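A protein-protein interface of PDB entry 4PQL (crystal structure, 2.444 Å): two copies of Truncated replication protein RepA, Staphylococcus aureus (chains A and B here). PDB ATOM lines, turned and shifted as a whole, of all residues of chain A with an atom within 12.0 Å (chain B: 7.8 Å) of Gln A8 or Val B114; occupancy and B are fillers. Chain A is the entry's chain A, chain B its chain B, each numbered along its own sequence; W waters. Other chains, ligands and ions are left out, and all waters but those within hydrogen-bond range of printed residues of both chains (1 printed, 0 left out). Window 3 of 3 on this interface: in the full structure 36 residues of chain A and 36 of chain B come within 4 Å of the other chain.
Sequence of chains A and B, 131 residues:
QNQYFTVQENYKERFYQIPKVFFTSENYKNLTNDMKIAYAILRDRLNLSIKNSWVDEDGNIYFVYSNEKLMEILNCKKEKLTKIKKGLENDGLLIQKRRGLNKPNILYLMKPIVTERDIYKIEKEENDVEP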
ATOM      1  N   GLN A   3      25.467  -1.158   3.719  1.00  0.00           N
ATOM      2  CA  GLN A   3      25.024  -1.686   4.988  1.00  0.00           C
ATOM      3  C   GLN A   3      23.662  -2.333   4.849  1.00  0.00           C
ATOM      4  O   GLN A   3      22.884  -2.005   3.953  1.00  0.00           O
ATOM      5  CB  GLN A   3      24.992  -0.592   6.055  1.00  0.00           C
ATOM      6  CG  GLN A   3      26.343  -0.308   6.688  1.00  0.00           C
ATOM      7  CD  GLN A   3      26.482   1.137   7.125  1.00  0.00           C
ATOM      8  OE1 GLN A   3      25.983   2.045   6.463  1.00  0.00           O
ATOM      9  NE2 GLN A   3      27.154   1.357   8.252  1.00  0.00           N
ATOM     10  N   TYR A   4      23.402  -3.287   5.728  1.00  0.00           N
ATOM     11  CA  TYR A   4      22.113  -3.935   5.784  1.00  0.00           C
ATOM     12  C   TYR A   4      21.112  -2.993   6.452  1.00  0.00           C
ATOM     13  O   TYR A   4      21.490  -1.995   7.074  1.00  0.00           O
ATOM     14  CB  TYR A   4      22.198  -5.247   6.563  1.00  0.00           C
ATOM     15  CG  TYR A   4      23.029  -6.319   5.900  1.00  0.00           C
ATOM     16  CD1 TYR A   4      24.412  -6.320   5.989  1.00  0.00           C
ATOM     17  CD2 TYR A   4      22.423  -7.344   5.192  1.00  0.00           C
ATOM     18  CE1 TYR A   4      25.165  -7.305   5.377  1.00  0.00           C
ATOM     19  CE2 TYR A   4      23.169  -8.333   4.568  1.00  0.00           C
ATOM     20  CZ  TYR A   4      24.538  -8.308   4.669  1.00  0.00           C
ATOM     21  OH  TYR A   4      25.267  -9.298   4.053  1.00  0.00           O
ATOM     22  N   PHE A   5      19.831  -3.280   6.274  1.00  0.00           N
ATOM     23  CA  PHE A   5      18.829  -2.667   7.119  1.00  0.00           C
ATOM     24  C   PHE A   5      18.726  -3.531   8.366  1.00  0.00           C
ATOM     25  O   PHE A   5      18.399  -4.716   8.272  1.00  0.00           O
ATOM     26  CB  PHE A   5      17.477  -2.579   6.416  1.00  0.00           C
ATOM     27  CG  PHE A   5      17.418  -1.548   5.322  1.00  0.00           C
ATOM     28  CD1 PHE A   5      17.643  -1.901   4.001  1.00  0.00           C
ATOM     29  CD2 PHE A   5      17.130  -0.226   5.617  1.00  0.00           C
ATOM     30  CE1 PHE A   5      17.580  -0.956   2.994  1.00  0.00           C
ATOM     31  CE2 PHE A   5      17.058   0.722   4.617  1.00  0.00           C
ATOM     32  CZ  PHE A   5      17.282   0.356   3.302  1.00  0.00           C
ATOM     33  N   THR A   6      19.004  -2.961   9.534  1.00  0.00           N
ATOM     34  CA  THR A   6      19.006  -3.766  10.753  1.00  0.00           C
ATOM     35  C   THR A   6      17.836  -3.371  11.646  1.00  0.00           C
ATOM     36  O   THR A   6      17.395  -2.208  11.644  1.00  0.00           O
ATOM     37  CB  THR A   6      20.301  -3.626  11.562  1.00  0.00           C
ATOM     38  OG1 THR A   6      20.296  -2.384  12.277  1.00  0.00           O
ATOM     39  CG2 THR A   6      21.538  -3.741  10.657  1.00  0.00           C
ATOM     40  N   VAL A   7      17.333  -4.351  12.391  1.00  0.00           N
ATOM     41  CA  VAL A   7      16.205  -4.158  13.286  1.00  0.00           C
ATOM     42  C   VAL A   7      16.586  -3.193  14.417  1.00  0.00           C
ATOM     43  O   VAL A   7      15.752  -2.400  14.889  1.00  0.00           O
ATOM     44  CB  VAL A   7      15.720  -5.530  13.849  1.00  0.00           C
ATOM     45  CG1 VAL A   7      16.754  -6.148  14.797  1.00  0.00           C
ATOM     46  CG2 VAL A   7      14.376  -5.400  14.528  1.00  0.00           C
ATOM     47  N   GLN A   8      17.860  -3.220  14.803  1.00  0.00           N
ATOM     48  CA  GLN A   8      18.383  -2.323  15.823  1.00  0.00           C
ATOM     49  C   GLN A   8      18.300  -0.880  15.344  1.00  0.00           C
ATOM     50  O   GLN A   8      17.867   0.020  16.075  1.00  0.00           O
ATOM     51  CB  GLN A   8      19.838  -2.671  16.145  1.00  0.00           C
ATOM     52  CG  GLN A   8      20.082  -4.131  16.498  1.00  0.00           C
ATOM     53  CD  GLN A   8      19.721  -4.460  17.933  1.00  0.00           C
ATOM     54  OE1 GLN A   8      19.275  -3.594  18.686  1.00  0.00           O
ATOM     55  NE2 GLN A   8      19.899  -5.727  18.319  1.00  0.00           N
ATOM     56  N   GLU A   9      18.710  -0.669  14.098  1.00  0.00           N
ATOM     57  CA  GLU A   9      18.666   0.655  13.513  1.00  0.00           C
ATOM     58  C   GLU A   9      17.217   1.094  13.349  1.00  0.00           C
ATOM     59  O   GLU A   9      16.888   2.255  13.551  1.00  0.00           O
ATOM     60  CB  GLU A   9      19.414   0.673  12.180  1.00  0.00           C
ATOM     61  CG  GLU A   9      19.596   2.053  11.590  1.00  0.00           C
ATOM     62  CD  GLU A   9      20.296   3.002  12.546  1.00  0.00           C
ATOM     63  OE1 GLU A   9      21.272   2.572  13.197  1.00  0.00           O
ATOM     64  OE2 GLU A   9      19.860   4.173  12.658  1.00  0.00           O
ATOM     65  N   ASN A  10      16.347   0.154  13.012  1.00  0.00           N
ATOM     66  CA  ASN A  10      14.935   0.465  12.845  1.00  0.00           C
ATOM     67  C   ASN A  10      14.307   0.987  14.128  1.00  0.00           C
ATOM     68  O   ASN A  10      13.593   1.990  14.110  1.00  0.00           O
ATOM     69  CB  ASN A  10      14.165  -0.749  12.350  1.00  0.00           C
ATOM     70  CG  ASN A  10      12.692  -0.447  12.118  1.00  0.00           C
ATOM     71  OD1 ASN A  10      11.882  -0.528  13.038  1.00  0.00           O
ATOM     72  ND2 ASN A  10      12.345  -0.089  10.891  1.00  0.00           N
ATOM     73  N   TYR A  11      14.547   0.297  15.238  1.00  0.00           N
ATOM     74  CA  TYR A  11      13.946   0.724  16.499  1.00  0.00           C
ATOM     75  C   TYR A  11      14.686   1.875  17.171  1.00  0.00           C
ATOM     76  O   TYR A  11      14.126   2.542  18.044  1.00  0.00           O
ATOM     77  CB  TYR A  11      13.802  -0.464  17.447  1.00  0.00           C
ATOM     78  CG  TYR A  11      12.661  -1.337  17.002  1.00  0.00           C
ATOM     79  CD1 TYR A  11      12.846  -2.349  16.067  1.00  0.00           C
ATOM     80  CD2 TYR A  11      11.374  -1.108  17.479  1.00  0.00           C
ATOM     81  CE1 TYR A  11      11.787  -3.123  15.641  1.00  0.00           C
ATOM     82  CE2 TYR A  11      10.313  -1.876  17.064  1.00  0.00           C
ATOM     83  CZ  TYR A  11      10.520  -2.876  16.146  1.00  0.00           C
ATOM     84  OH  TYR A  11       9.453  -3.630  15.733  1.00  0.00           O
ATOM     85  N   LYS A  12      15.927   2.121  16.758  1.00  0.00           N
ATOM     86  CA  LYS A  12      16.623   3.339  17.166  1.00  0.00           C
ATOM     87  C   LYS A  12      15.940   4.573  16.581  1.00  0.00           C
ATOM     88  O   LYS A  12      15.962   5.648  17.175  1.00  0.00           O
ATOM     89  CB  LYS A  12      18.087   3.290  16.728  1.00  0.00           C
ATOM     90  CG  LYS A  12      19.042   2.956  17.848  1.00  0.00           C
ATOM     91  CD  LYS A  12      20.433   2.701  17.326  1.00  0.00           C
ATOM     92  CE  LYS A  12      21.084   1.587  18.116  1.00  0.00           C
ATOM     93  NZ  LYS A  12      22.363   1.165  17.490  1.00  0.00           N
ATOM     94  N   GLU A  13      15.303   4.390  15.429  1.00  0.00           N
ATOM     95  CA  GLU A  13      14.668   5.478  14.703  1.00  0.00           C
ATOM     96  C   GLU A  13      13.148   5.510  14.877  1.00  0.00           C
ATOM     97  O   GLU A  13      12.425   5.857  13.947  1.00  0.00           O
ATOM     98  CB  GLU A  13      15.025   5.397  13.214  1.00  0.00           C
ATOM     99  CG  GLU A  13      16.489   5.667  12.911  1.00  0.00           C
ATOM    100  CD  GLU A  13      16.904   7.100  13.243  1.00  0.00           C
ATOM    101  OE1 GLU A  13      16.352   8.042  12.626  1.00  0.00           O
ATOM    102  OE2 GLU A  13      17.779   7.289  14.118  1.00  0.00           O
ATOM    103  N   ARG A  14      12.672   5.121  16.059  1.00  0.00           N
ATOM    104  CA  ARG A  14      11.256   5.246  16.422  1.00  0.00           C
ATOM    105  C   ARG A  14      11.105   6.368  17.445  1.00  0.00           C
ATOM    106  O   ARG A  14      11.786   6.359  18.470  1.00  0.00           O
ATOM    107  CB  ARG A  14      10.718   3.944  17.019  1.00  0.00           C
ATOM    108  CG  ARG A  14      10.960   2.672  16.203  1.00  0.00           C
ATOM    109  CD  ARG A  14       9.937   2.416  15.105  1.00  0.00           C
ATOM    110  NE  ARG A  14       9.930   0.995  14.737  1.00  0.00           N
ATOM    111  CZ  ARG A  14       9.031   0.413  13.943  1.00  0.00           C
ATOM    112  NH1 ARG A  14       8.029   1.119  13.428  1.00  0.00           N
ATOM    113  NH2 ARG A  14       9.121  -0.886  13.677  1.00  0.00           N
ATOM    114  N   PHE A  15      10.215   7.323  17.189  1.00  0.00           N
ATOM    115  CA  PHE A  15      10.129   8.499  18.057  1.00  0.00           C
ATOM    116  C   PHE A  15       8.719   8.848  18.505  1.00  0.00           C
ATOM    117  O   PHE A  15       7.727   8.460  17.883  1.00  0.00           O
ATOM    118  CB  PHE A  15      10.729   9.731  17.357  1.00  0.00           C
ATOM    119  CG  PHE A  15      12.109   9.506  16.812  1.00  0.00           C
ATOM    120  CD1 PHE A  15      12.299   9.213  15.471  1.00  0.00           C
ATOM    121  CD2 PHE A  15      13.214   9.573  17.642  1.00  0.00           C
ATOM    122  CE1 PHE A  15      13.572   8.991  14.965  1.00  0.00           C
ATOM    123  CE2 PHE A  15      14.488   9.354  17.145  1.00  0.00           C
ATOM    124  CZ  PHE A  15      14.666   9.066  15.804  1.00  0.00           C
ATOM    125  N   PRO B  19      13.270   9.525  21.266  1.00  0.00           N
ATOM    126  CA  PRO B  19      13.329   8.087  20.977  1.00  0.00           C
ATOM    127  C   PRO B  19      12.425   7.303  21.912  1.00  0.00           C
ATOM    128  O   PRO B  19      12.395   7.558  23.117  1.00  0.00           O
ATOM    129  CB  PRO B  19      14.806   7.740  21.201  1.00  0.00           C
ATOM    130  CG  PRO B  19      15.540   9.029  21.050  1.00  0.00           C
ATOM    131  CD  PRO B  19      14.601  10.082  21.571  1.00  0.00           C
ATOM    132  N   LYS B  20      11.684   6.356  21.362  1.00  0.00           N
ATOM    133  CA  LYS B  20      10.726   5.616  22.164  1.00  0.00           C
ATOM    134  C   LYS B  20      11.400   4.809  23.271  1.00  0.00           C
ATOM    135  O   LYS B  20      10.813   4.598  24.332  1.00  0.00           O
ATOM    136  CB  LYS B  20       9.901   4.696  21.275  1.00  0.00           C
ATOM    137  CG  LYS B  20       8.813   5.408  20.501  1.00  0.00           C
ATOM    138  CD  LYS B  20       8.038   4.421  19.654  1.00  0.00           C
ATOM    139  CE  LYS B  20       6.857   5.069  18.961  1.00  0.00           C
ATOM    140  NZ  LYS B  20       5.797   4.051  18.735  1.00  0.00           N
ATOM    141  N   VAL B  21      12.649   4.411  23.047  1.00  0.00           N
ATOM    142  CA  VAL B  21      13.378   3.604  24.018  1.00  0.00           C
ATOM    143  C   VAL B  21      13.601   4.343  25.342  1.00  0.00           C
ATOM    144  O   VAL B  21      13.726   3.711  26.395  1.00  0.00           O
ATOM    145  CB  VAL B  21      14.745   3.140  23.439  1.00  0.00           C
ATOM    146  CG1 VAL B  21      15.717   4.306  23.305  1.00  0.00           C
ATOM    147  CG2 VAL B  21      15.338   2.043  24.295  1.00  0.00           C
ATOM    148  N   THR B  24      11.000   2.921  27.435  1.00  0.00           N
ATOM    149  CA  THR B  24      10.904   1.471  27.667  1.00  0.00           C
ATOM    150  C   THR B  24      12.107   0.908  28.419  1.00  0.00           C
ATOM    151  O   THR B  24      11.958   0.056  29.295  1.00  0.00           O
ATOM    152  CB  THR B  24      10.729   0.688  26.357  1.00  0.00           C
ATOM    153  OG1 THR B  24      11.910   0.812  25.559  1.00  0.00           O
ATOM    154  CG2 THR B  24       9.534   1.219  25.584  1.00  0.00           C
ATOM    155  N   SER B  25      13.295   1.367  28.056  1.00  0.00           N
ATOM    156  CA  SER B  25      14.528   0.824  28.602  1.00  0.00           C
ATOM    157  C   SER B  25      14.726   1.157  30.075  1.00  0.00           C
ATOM    158  O   SER B  25      14.491   2.285  30.515  1.00  0.00           O
ATOM    159  CB  SER B  25      15.730   1.342  27.813  1.00  0.00           C
ATOM    160  OG  SER B  25      16.935   0.782  28.308  1.00  0.00           O
ATOM    161  N   ASN B  27      17.574   1.197  31.245  1.00  0.00           N
ATOM    162  CA  ASN B  27      18.786   1.995  31.156  1.00  0.00           C
ATOM    163  C   ASN B  27      18.549   3.505  31.117  1.00  0.00           C
ATOM    164  O   ASN B  27      19.370   4.277  31.615  1.00  0.00           O
ATOM    165  CB  ASN B  27      19.565   1.591  29.907  1.00  0.00           C
ATOM    166  CG  ASN B  27      20.114   0.178  29.987  1.00  0.00           C
ATOM    167  OD1 ASN B  27      20.424  -0.326  31.070  1.00  0.00           O
ATOM    168  ND2 ASN B  27      20.236  -0.471  28.833  1.00  0.00           N
ATOM    169  N   TYR B  28      17.436   3.927  30.524  1.00  0.00           N
ATOM    170  CA  TYR B  28      17.153   5.354  30.380  1.00  0.00           C
ATOM    171  C   TYR B  28      16.049   5.806  31.323  1.00  0.00           C
ATOM    172  O   TYR B  28      15.519   6.908  31.185  1.00  0.00           O
ATOM    173  CB  TYR B  28      16.790   5.697  28.932  1.00  0.00           C
ATOM    174  CG  TYR B  28      17.855   5.298  27.937  1.00  0.00           C
ATOM    175  CD1 TYR B  28      17.576   4.412  26.908  1.00  0.00           C
ATOM    176  CD2 TYR B  28      19.154   5.791  28.050  1.00  0.00           C
ATOM    177  CE1 TYR B  28      18.555   4.039  26.006  1.00  0.00           C
ATOM    178  CE2 TYR B  28      20.139   5.427  27.155  1.00  0.00           C
ATOM    179  CZ  TYR B  28      19.836   4.551  26.132  1.00  0.00           C
ATOM    180  OH  TYR B  28      20.808   4.182  25.239  1.00  0.00           O
ATOM    181  N   LYS B 111      23.447   8.272  19.611  1.00  0.00           N
ATOM    182  CA  LYS B 111      22.269   7.442  19.449  1.00  0.00           C
ATOM    183  C   LYS B 111      22.105   6.590  20.698  1.00  0.00           C
ATOM    184  O   LYS B 111      23.096   6.210  21.322  1.00  0.00           O
ATOM    185  CB  LYS B 111      22.397   6.546  18.217  1.00  0.00           C
ATOM    186  CG  LYS B 111      22.485   7.272  16.894  1.00  0.00           C
ATOM    187  CD  LYS B 111      22.880   6.295  15.800  1.00  0.00           C
ATOM    188  CE  LYS B 111      21.971   6.390  14.592  1.00  0.00           C
ATOM    189  NZ  LYS B 111      22.124   7.710  13.907  1.00  0.00           N
ATOM    190  N   PRO B 112      20.856   6.283  21.074  1.00  0.00           N
ATOM    191  CA  PRO B 112      20.587   5.406  22.220  1.00  0.00           C
ATOM    192  C   PRO B 112      20.868   3.938  21.902  1.00  0.00           C
ATOM    193  O   PRO B 112      21.028   3.594  20.733  1.00  0.00           O
ATOM    194  CB  PRO B 112      19.093   5.625  22.488  1.00  0.00           C
ATOM    195  CG  PRO B 112      18.534   6.019  21.161  1.00  0.00           C
ATOM    196  CD  PRO B 112      19.616   6.804  20.467  1.00  0.00           C
ATOM    197  N   ILE B 113      20.917   3.097  22.933  1.00  0.00           N
ATOM    198  CA  ILE B 113      21.058   1.647  22.781  1.00  0.00           C
ATOM    199  C   ILE B 113      19.694   0.973  22.779  1.00  0.00           C
ATOM    200  O   ILE B 113      18.837   1.286  23.607  1.00  0.00           O
ATOM    201  CB  ILE B 113      21.890   1.009  23.925  1.00  0.00           C
ATOM    202  CG1 ILE B 113      23.348   1.380  23.821  1.00  0.00           C
ATOM    203  CG2 ILE B 113      21.816  -0.504  23.881  1.00  0.00           C
ATOM    204  CD1 ILE B 113      24.132   1.186  25.106  1.00  0.00           C
ATOM    205  N   VAL B 114      19.488   0.050  21.849  1.00  0.00           N
ATOM    206  CA  VAL B 114      18.232  -0.683  21.804  1.00  0.00           C
ATOM    207  C   VAL B 114      18.446  -2.176  22.053  1.00  0.00           C
ATOM    208  O   VAL B 114      19.203  -2.833  21.343  1.00  0.00           O
ATOM    209  CB  VAL B 114      17.531  -0.493  20.449  1.00  0.00           C
ATOM    210  CG1 VAL B 114      16.233  -1.268  20.409  1.00  0.00           C
ATOM    211  CG2 VAL B 114      17.280   0.975  20.195  1.00  0.00           C
ATOM    212  N   THR B 115      17.768  -2.708  23.066  1.00  0.00           N
ATOM    213  CA  THR B 115      17.861  -4.132  23.373  1.00  0.00           C
ATOM    214  C   THR B 115      16.610  -4.873  22.924  1.00  0.00           C
ATOM    215  O   THR B 115      15.623  -4.255  22.515  1.00  0.00           O
ATOM    216  CB  THR B 115      18.071  -4.387  24.883  1.00  0.00           C
ATOM    217  OG1 THR B 115      16.856  -4.096  25.594  1.00  0.00           O
ATOM    218  CG2 THR B 115      19.208  -3.521  25.429  1.00  0.00           C
ATOM    219  N   GLU B 116      16.651  -6.198  23.016  1.00  0.00           N
ATOM    220  CA  GLU B 116      15.512  -7.022  22.639  1.00  0.00           C
ATOM    221  C   GLU B 116      14.300  -6.725  23.509  1.00  0.00           C
ATOM    222  O   GLU B 116      13.178  -6.796  23.033  1.00  0.00           O
ATOM    223  CB  GLU B 116      15.870  -8.508  22.692  1.00  0.00           C
ATOM    224  CG  GLU B 116      16.816  -8.922  21.578  1.00  0.00           C
ATOM    225  CD  GLU B 116      16.244 -10.020  20.697  1.00  0.00           C
ATOM    226  OE1 GLU B 116      15.396 -10.804  21.177  1.00  0.00           O
ATOM    227  OE2 GLU B 116      16.637 -10.088  19.510  1.00  0.00           O
ATOM    228  N   ARG B 117      14.518  -6.412  24.783  1.00  0.00           N
ATOM    229  CA  ARG B 117      13.411  -6.027  25.656  1.00  0.00           C
ATOM    230  C   ARG B 117      12.766  -4.730  25.160  1.00  0.00           C
ATOM    231  O   ARG B 117      11.536  -4.594  25.158  1.00  0.00           O
ATOM    232  CB  ARG B 117      13.883  -5.867  27.103  1.00  0.00           C
ATOM    233  CG  ARG B 117      14.240  -7.183  27.782  1.00  0.00           C
ATOM    234  CD  ARG B 117      13.671  -7.277  29.193  1.00  0.00           C
ATOM    235  NE  ARG B 117      12.208  -7.256  29.184  1.00  0.00           N
ATOM    236  CZ  ARG B 117      11.448  -7.204  30.274  1.00  0.00           C
ATOM    237  NH1 ARG B 117      12.006  -7.172  31.476  1.00  0.00           N
ATOM    238  NH2 ARG B 117      10.125  -7.189  30.159  1.00  0.00           N
ATOM    239  N   ASP B 118      13.604  -3.797  24.708  1.00  0.00           N
ATOM    240  CA  ASP B 118      13.139  -2.529  24.149  1.00  0.00           C
ATOM    241  C   ASP B 118      12.325  -2.779  22.896  1.00  0.00           C
ATOM    242  O   ASP B 118      11.217  -2.264  22.750  1.00  0.00           O
ATOM    243  CB  ASP B 118      14.326  -1.623  23.801  1.00  0.00           C
ATOM    244  CG  ASP B 118      15.164  -1.269  25.002  1.00  0.00           C
ATOM    245  OD1 ASP B 118      14.605  -1.084  26.095  1.00  0.00           O
ATOM    246  OD2 ASP B 118      16.400  -1.210  24.864  1.00  0.00           O
ATOM    247  N   ILE B 119      12.874  -3.608  22.010  1.00  0.00           N
ATOM    248  CA  ILE B 119      12.223  -3.945  20.751  1.00  0.00           C
ATOM    249  C   ILE B 119      10.875  -4.628  20.991  1.00  0.00           C
ATOM    250  O   ILE B 119       9.881  -4.310  20.336  1.00  0.00           O
ATOM    251  CB  ILE B 119      13.129  -4.869  19.900  1.00  0.00           C
ATOM    252  CG1 ILE B 119      14.405  -4.127  19.502  1.00  0.00           C
ATOM    253  CG2 ILE B 119      12.402  -5.376  18.658  1.00  0.00           C
ATOM    254  CD1 ILE B 119      15.361  -4.953  18.662  1.00  0.00           C
ATOM    255  N   TYR B 120      10.851  -5.560  21.937  1.00  0.00           N
ATOM    256  CA  TYR B 120       9.633  -6.285  22.254  1.00  0.00           C
ATOM    257  C   TYR B 120       8.573  -5.331  22.789  1.00  0.00           C
ATOM    258  O   TYR B 120       7.439  -5.348  22.322  1.00  0.00           O
ATOM    259  CB  TYR B 120       9.903  -7.404  23.260  1.00  0.00           C
ATOM    260  CG  TYR B 120       8.647  -8.007  23.853  1.00  0.00           C
ATOM    261  CD1 TYR B 120       7.936  -8.988  23.172  1.00  0.00           C
ATOM    262  CD2 TYR B 120       8.175  -7.599  25.096  1.00  0.00           C
ATOM    263  CE1 TYR B 120       6.786  -9.546  23.709  1.00  0.00           C
ATOM    264  CE2 TYR B 120       7.025  -8.146  25.641  1.00  0.00           C
ATOM    265  CZ  TYR B 120       6.335  -9.121  24.946  1.00  0.00           C
ATOM    266  OH  TYR B 120       5.194  -9.670  25.490  1.00  0.00           O
ATOM    267  N   ILE B 122       8.326  -2.031  22.463  1.00  0.00           N
ATOM    268  CA  ILE B 122       7.891  -1.108  21.431  1.00  0.00           C
ATOM    269  C   ILE B 122       6.972  -1.813  20.434  1.00  0.00           C
ATOM    270  O   ILE B 122       5.975  -1.237  20.015  1.00  0.00           O
ATOM    271  CB  ILE B 122       9.071  -0.468  20.692  1.00  0.00           C
ATOM    272  CG1 ILE B 122       9.886   0.390  21.662  1.00  0.00           C
ATOM    273  CG2 ILE B 122       8.565   0.421  19.577  1.00  0.00           C
ATOM    274  CD1 ILE B 122      11.219   0.846  21.120  1.00  0.00           C
HETATM  275  O   HOH W   1      13.425   4.294  19.800  1.00  0.00           O
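The backbone carbonyl oxygen of Arg A14 lies within hydrogen-bond range of the backbone NH of Lys B20 (2.9 Å).
O of Val B114 sits close to OE1 of Gln A8 (2.8 Å).
Glu A9 touches Lys B111 (OE2 to CE, 3.6 Å).
CB of Tyr A11 touches CG1 of Val B114, 3.9 Å away.
Ile B119 touches Tyr A11 (CG2 to CE1, 3.8 Å).
CD2 of Tyr A11 touches CG2 of Ile B122, at 3.8 Å.
CE of Lys A12 touches O of Pro B112 (3.3 Å).
CG of Lys A12 touches CG2 of Val B114, at 3.5 Å.
CA of Pro B19 touches O of Arg A14, at 3.4 Å.
N of Pro B19 touches CD2 of Phe A15 (3.6 Å).
Lys B20 touches Phe A15.
The guanidinium group of Arg A14 lies within hydrogen-bond range of the side-chain hydroxyl of Tyr A11 (3.4 Å).
The side-chain amide oxygen of Asn A10 lies within hydrogen-bond range of the guanidinium group of Arg A14 (2.9 Å).
The backbone NH (N) of Glu A9 sits at hydrogen-bond distance from the side-chain hydroxyl (OG1) of Thr A6 (3.0 Å).
Hydrophobic or aromatic side chains of chain A that line the printed part of chain B: Tyr A11 and Phe A15.
Among the printed residues, no Asp or Glu carboxylate lies within 4 Å of a Lys or Arg side-chain nitrogen of the other chain.
No position is printed for both chains.
Of the 11 pairs that touch across the chains among the printed residues, none has its exchanged pair printed and touching as well.
Water W1 lies within hydrogen-bond range of the backbone carbonyl oxygen (O) of Tyr A11 (2.6 Å), the backbone carbonyl oxygen (O) of Arg A14 (3.0 Å), the backbone NH (N) of Lys B20 (3.1 Å) and the backbone NH (N) of Val B21 (3.3 Å).
Of the printed residues of chain B, Phe A15 touches Pro B19 and Lys B20.
Of the printed residues of chain A, Pro B19 touches Arg A14 and Phe A15.
Printed residues of chain A within 4 Å of Lys B20: Arg A14 (2.9 Å) and Phe A15 (3.7 Å).
No residue of chain A comes within 4 Å of Ile B113.
Of the printed residues of chain A, Val B114 touches Gln A8, Tyr A11 and Lys A12.
No residue of chain A comes within 4 Å of Asp B118.
Of chain A, only Tyr A11 (3.8 Å) comes within 4 Å of Ile B119.
The nearest printed residue of chain B that does not touch Tyr A11 is Asp B118 (5.4 Å).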
